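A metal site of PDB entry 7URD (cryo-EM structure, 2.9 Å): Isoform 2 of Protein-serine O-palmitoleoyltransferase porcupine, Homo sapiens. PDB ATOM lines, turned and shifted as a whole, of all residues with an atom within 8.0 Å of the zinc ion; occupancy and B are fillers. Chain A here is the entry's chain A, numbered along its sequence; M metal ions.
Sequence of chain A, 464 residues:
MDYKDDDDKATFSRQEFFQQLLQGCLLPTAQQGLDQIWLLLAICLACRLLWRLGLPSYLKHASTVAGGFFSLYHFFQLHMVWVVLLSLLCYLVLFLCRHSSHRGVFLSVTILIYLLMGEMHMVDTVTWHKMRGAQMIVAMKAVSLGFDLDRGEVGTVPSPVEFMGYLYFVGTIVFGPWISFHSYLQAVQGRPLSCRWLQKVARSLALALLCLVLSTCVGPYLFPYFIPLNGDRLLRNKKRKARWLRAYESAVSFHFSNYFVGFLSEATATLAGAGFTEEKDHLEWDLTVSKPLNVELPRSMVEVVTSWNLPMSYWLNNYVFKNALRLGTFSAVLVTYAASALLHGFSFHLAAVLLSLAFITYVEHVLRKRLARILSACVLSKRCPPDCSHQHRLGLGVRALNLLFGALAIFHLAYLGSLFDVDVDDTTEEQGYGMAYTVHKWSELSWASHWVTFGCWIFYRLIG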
ATOM      1  N   ARG A 299      23.375   0.276  14.343  1.00  0.00           N
ATOM      2  CA  ARG A 299      23.206  -1.166  14.399  1.00  0.00           C
ATOM      3  C   ARG A 299      23.265  -1.785  13.014  1.00  0.00           C
ATOM      4  O   ARG A 299      23.804  -2.882  12.835  1.00  0.00           O
ATOM      5  CB  ARG A 299      21.893  -1.522  15.076  1.00  0.00           C
ATOM      6  CG  ARG A 299      21.675  -3.008  15.243  1.00  0.00           C
ATOM      7  CD  ARG A 299      20.240  -3.323  15.608  1.00  0.00           C
ATOM      8  NE  ARG A 299      19.973  -4.755  15.541  1.00  0.00           N
ATOM      9  CZ  ARG A 299      20.033  -5.572  16.581  1.00  0.00           C
ATOM     10  NH1 ARG A 299      20.336  -5.099  17.775  1.00  0.00           N
ATOM     11  NH2 ARG A 299      19.777  -6.868  16.420  1.00  0.00           N
ATOM     12  N   ALA A 372      19.838 -14.807  10.980  1.00  0.00           N
ATOM     13  CA  ALA A 372      19.006 -14.995  12.161  1.00  0.00           C
ATOM     14  C   ALA A 372      18.071 -16.190  12.010  1.00  0.00           C
ATOM     15  O   ALA A 372      17.656 -16.763  13.011  1.00  0.00           O
ATOM     16  CB  ALA A 372      18.199 -13.728  12.436  1.00  0.00           C
ATOM     17  N   SER A 376      19.434 -19.031  14.482  1.00  0.00           N
ATOM     18  CA  SER A 376      18.389 -18.817  15.486  1.00  0.00           C
ATOM     19  C   SER A 376      18.811 -17.790  16.522  1.00  0.00           C
ATOM     20  O   SER A 376      18.500 -17.908  17.712  1.00  0.00           O
ATOM     21  CB  SER A 376      17.977 -20.131  16.155  1.00  0.00           C
ATOM     22  OG  SER A 376      16.958 -19.918  17.109  1.00  0.00           O
ATOM     23  N   ALA A 377      19.599 -16.813  16.107  1.00  0.00           N
ATOM     24  CA  ALA A 377      20.043 -15.774  17.019  1.00  0.00           C
ATOM     25  C   ALA A 377      19.336 -14.488  16.666  1.00  0.00           C
ATOM     26  O   ALA A 377      18.876 -14.334  15.551  1.00  0.00           O
ATOM     27  CB  ALA A 377      21.546 -15.591  16.924  1.00  0.00           C
ATOM     28  N   CYS A 378      19.222 -13.576  17.616  1.00  0.00           N
ATOM     29  CA  CYS A 378      18.561 -12.314  17.320  1.00  0.00           C
ATOM     30  C   CYS A 378      19.530 -11.301  16.736  1.00  0.00           C
ATOM     31  O   CYS A 378      19.890 -10.331  17.397  1.00  0.00           O
ATOM     32  CB  CYS A 378      17.848 -11.774  18.564  1.00  0.00           C
ATOM     33  SG  CYS A 378      16.125 -12.307  18.719  1.00  0.00           S
ATOM     34  N   VAL A 379      19.950 -11.527  15.499  1.00  0.00           N
ATOM     35  CA  VAL A 379      20.865 -10.644  14.801  1.00  0.00           C
ATOM     36  C   VAL A 379      20.187  -9.859  13.685  1.00  0.00           C
ATOM     37  O   VAL A 379      20.859  -9.316  12.835  1.00  0.00           O
ATOM     38  CB  VAL A 379      22.041 -11.392  14.181  1.00  0.00           C
ATOM     39  CG1 VAL A 379      22.604 -12.393  15.162  1.00  0.00           C
ATOM     40  CG2 VAL A 379      21.593 -12.108  12.924  1.00  0.00           C
ATOM     41  N   LEU A 380      18.860  -9.823  13.683  1.00  0.00           N
ATOM     42  CA  LEU A 380      18.091  -9.114  12.665  1.00  0.00           C
ATOM     43  C   LEU A 380      18.447  -7.633  12.579  1.00  0.00           C
ATOM     44  O   LEU A 380      18.747  -6.992  13.575  1.00  0.00           O
ATOM     45  CB  LEU A 380      16.608  -9.300  12.890  1.00  0.00           C
ATOM     46  CG  LEU A 380      16.142 -10.700  12.518  1.00  0.00           C
ATOM     47  CD1 LEU A 380      14.636 -10.772  12.513  1.00  0.00           C
ATOM     48  CD2 LEU A 380      16.682 -11.037  11.140  1.00  0.00           C
ATOM     49  N   LYS A 382      17.012  -5.125  12.791  1.00  0.00           N
ATOM     50  CA  LYS A 382      16.373  -4.298  13.795  1.00  0.00           C
ATOM     51  C   LYS A 382      16.173  -5.130  15.051  1.00  0.00           C
ATOM     52  O   LYS A 382      16.116  -6.364  14.993  1.00  0.00           O
ATOM     53  CB  LYS A 382      15.019  -3.750  13.312  1.00  0.00           C
ATOM     54  CG  LYS A 382      15.129  -2.700  12.228  1.00  0.00           C
ATOM     55  CD  LYS A 382      13.925  -1.776  12.238  1.00  0.00           C
ATOM     56  CE  LYS A 382      14.020  -0.716  11.146  1.00  0.00           C
ATOM     57  NZ  LYS A 382      13.809  -1.313   9.796  1.00  0.00           N
ATOM     58  N   ARG A 383      16.073  -4.457  16.189  1.00  0.00           N
ATOM     59  CA  ARG A 383      15.945  -5.151  17.463  1.00  0.00           C
ATOM     60  C   ARG A 383      14.665  -5.973  17.489  1.00  0.00           C
ATOM     61  O   ARG A 383      13.570  -5.469  17.207  1.00  0.00           O
ATOM     62  CB  ARG A 383      15.963  -4.158  18.616  1.00  0.00           C
ATOM     63  CG  ARG A 383      17.355  -3.812  19.106  1.00  0.00           C
ATOM     64  CD  ARG A 383      17.339  -2.700  20.126  1.00  0.00           C
ATOM     65  NE  ARG A 383      18.644  -2.492  20.726  1.00  0.00           N
ATOM     66  CZ  ARG A 383      18.979  -1.417  21.444  1.00  0.00           C
ATOM     67  NH1 ARG A 383      18.093  -0.454  21.652  1.00  0.00           N
ATOM     68  NH2 ARG A 383      20.200  -1.312  21.946  1.00  0.00           N
ATOM     69  N   CYS A 384      14.798  -7.243  17.868  1.00  0.00           N
ATOM     70  CA  CYS A 384      13.658  -8.130  17.945  1.00  0.00           C
ATOM     71  C   CYS A 384      12.756  -7.813  19.110  1.00  0.00           C
ATOM     72  O   CYS A 384      13.211  -7.386  20.161  1.00  0.00           O
ATOM     73  CB  CYS A 384      14.152  -9.554  18.101  1.00  0.00           C
ATOM     74  SG  CYS A 384      14.216 -10.425  16.533  1.00  0.00           S
ATOM     75  N   PRO A 385      11.449  -8.040  18.933  1.00  0.00           N
ATOM     76  CA  PRO A 385      10.455  -7.826  19.988  1.00  0.00           C
ATOM     77  C   PRO A 385      10.587  -8.922  21.033  1.00  0.00           C
ATOM     78  O   PRO A 385      11.064 -10.011  20.733  1.00  0.00           O
ATOM     79  CB  PRO A 385       9.133  -7.961  19.243  1.00  0.00           C
ATOM     80  CG  PRO A 385       9.438  -8.788  18.048  1.00  0.00           C
ATOM     81  CD  PRO A 385      10.841  -8.430  17.649  1.00  0.00           C
ATOM     82  N   PRO A 386      10.136  -8.652  22.259  1.00  0.00           N
ATOM     83  CA  PRO A 386      10.242  -9.565  23.414  1.00  0.00           C
ATOM     84  C   PRO A 386       9.731 -11.020  23.251  1.00  0.00           C
ATOM     85  O   PRO A 386      10.219 -11.888  23.974  1.00  0.00           O
ATOM     86  CB  PRO A 386       9.427  -8.842  24.487  1.00  0.00           C
ATOM     87  CG  PRO A 386       9.512  -7.397  24.123  1.00  0.00           C
ATOM     88  CD  PRO A 386       9.496  -7.383  22.622  1.00  0.00           C
ATOM     89  N   ASP A 387       8.804 -11.252  22.339  1.00  0.00           N
ATOM     90  CA  ASP A 387       8.278 -12.595  22.126  1.00  0.00           C
ATOM     91  C   ASP A 387       8.753 -13.148  20.791  1.00  0.00           C
ATOM     92  O   ASP A 387       7.997 -13.170  19.828  1.00  0.00           O
ATOM     93  CB  ASP A 387       6.748 -12.586  22.146  1.00  0.00           C
ATOM     94  CG  ASP A 387       6.172 -12.042  23.437  1.00  0.00           C
ATOM     95  OD1 ASP A 387       6.906 -11.972  24.451  1.00  0.00           O
ATOM     96  OD2 ASP A 387       4.970 -11.691  23.454  1.00  0.00           O
ATOM     97  N   CYS A 388      10.001 -13.603  20.728  1.00  0.00           N
ATOM     98  CA  CYS A 388      10.528 -14.137  19.468  1.00  0.00           C
ATOM     99  C   CYS A 388      11.173 -15.514  19.574  1.00  0.00           C
ATOM    100  O   CYS A 388      11.767 -15.863  20.588  1.00  0.00           O
ATOM    101  CB  CYS A 388      11.498 -13.148  18.852  1.00  0.00           C
ATOM    102  SG  CYS A 388      13.219 -13.380  19.352  1.00  0.00           S
ATOM    103  N   SER A 389      11.047 -16.271  18.503  1.00  0.00           N
ATOM    104  CA  SER A 389      11.563 -17.637  18.421  1.00  0.00           C
ATOM    105  C   SER A 389      13.056 -17.826  18.633  1.00  0.00           C
ATOM    106  O   SER A 389      13.479 -18.924  19.015  1.00  0.00           O
ATOM    107  CB  SER A 389      11.162 -18.256  17.075  1.00  0.00           C
ATOM    108  OG  SER A 389      11.894 -17.674  16.016  1.00  0.00           O
ATOM    109  N   HIS A 390      13.877 -16.816  18.370  1.00  0.00           N
ATOM    110  CA  HIS A 390      15.325 -16.993  18.534  1.00  0.00           C
ATOM    111  C   HIS A 390      15.801 -17.529  19.874  1.00  0.00           C
ATOM    112  O   HIS A 390      15.368 -17.064  20.922  1.00  0.00           O
ATOM    113  CB  HIS A 390      16.050 -15.697  18.197  1.00  0.00           C
ATOM    114  CG  HIS A 390      15.678 -15.115  16.871  1.00  0.00           C
ATOM    115  ND1 HIS A 390      14.986 -13.938  16.745  1.00  0.00           N
ATOM    116  CD2 HIS A 390      15.883 -15.574  15.616  1.00  0.00           C
ATOM    117  CE1 HIS A 390      14.784 -13.691  15.468  1.00  0.00           C
ATOM    118  NE2 HIS A 390      15.316 -14.671  14.763  1.00  0.00           N
ATOM    119  N   GLN A 391      16.701 -18.500  19.825  1.00  0.00           N
ATOM    120  CA  GLN A 391      17.199 -19.139  21.042  1.00  0.00           C
ATOM    121  C   GLN A 391      18.289 -18.303  21.706  1.00  0.00           C
ATOM    122  O   GLN A 391      18.146 -17.886  22.868  1.00  0.00           O
ATOM    123  CB  GLN A 391      17.721 -20.545  20.725  1.00  0.00           C
ATOM    124  CG  GLN A 391      16.635 -21.519  20.298  1.00  0.00           C
ATOM    125  CD  GLN A 391      17.182 -22.884  19.961  1.00  0.00           C
ATOM    126  OE1 GLN A 391      18.393 -23.105  19.994  1.00  0.00           O
ATOM    127  NE2 GLN A 391      16.283 -23.819  19.655  1.00  0.00           N
ATOM    128  N   HIS A 392      19.377 -18.037  20.985  1.00  0.00           N
ATOM    129  CA  HIS A 392      20.477 -17.236  21.512  1.00  0.00           C
ATOM    130  C   HIS A 392      20.127 -15.761  21.303  1.00  0.00           C
ATOM    131  O   HIS A 392      20.264 -15.232  20.196  1.00  0.00           O
ATOM    132  CB  HIS A 392      21.785 -17.593  20.824  1.00  0.00           C
ATOM    133  CG  HIS A 392      22.038 -19.076  20.759  1.00  0.00           C
ATOM    134  ND1 HIS A 392      21.609 -19.849  19.713  1.00  0.00           N
ATOM    135  CD2 HIS A 392      22.665 -19.906  21.618  1.00  0.00           C
ATOM    136  CE1 HIS A 392      21.969 -21.109  19.931  1.00  0.00           C
ATOM    137  NE2 HIS A 392      22.610 -21.164  21.082  1.00  0.00           N
ATOM    138  N   ARG A 393      19.677 -15.100  22.361  1.00  0.00           N
ATOM    139  CA  ARG A 393      19.260 -13.708  22.294  1.00  0.00           C
ATOM    140  C   ARG A 393      20.291 -12.757  22.893  1.00  0.00           C
ATOM    141  O   ARG A 393      20.664 -11.768  22.252  1.00  0.00           O
ATOM    142  CB  ARG A 393      17.920 -13.525  23.017  1.00  0.00           C
ATOM    143  CG  ARG A 393      16.820 -14.435  22.501  1.00  0.00           C
ATOM    144  CD  ARG A 393      15.531 -14.235  23.274  1.00  0.00           C
ATOM    145  NE  ARG A 393      14.484 -15.161  22.834  1.00  0.00           N
ATOM    146  CZ  ARG A 393      13.287 -15.251  23.391  1.00  0.00           C
ATOM    147  NH1 ARG A 393      12.970 -14.474  24.421  1.00  0.00           N
ATOM    148  NH2 ARG A 393      12.406 -16.122  22.933  1.00  0.00           N
HETATM  149 ZN    ZN M   1      14.325 -12.175  17.724  1.00  0.00          ZN
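The backbone NH (N) of Cys 378 sits at hydrogen-bond distance from the backbone carbonyl oxygen (O) of His 392, 3.2 Å away.
NE of Arg 393 is in hydrogen-bond range of O of His 390.
The guanidinium group (NH2) of Arg 393 is in hydrogen-bond range of the backbone carbonyl oxygen (O) of Cys 388.
The zinc ion is bound by the side-chain sulfur of Cys 378, the side-chain sulfur of Cys 384, a ring nitrogen (ND1) of His 390 and the side-chain sulfur of Cys 388.
The zinc ion has four donor atoms within binding distance.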
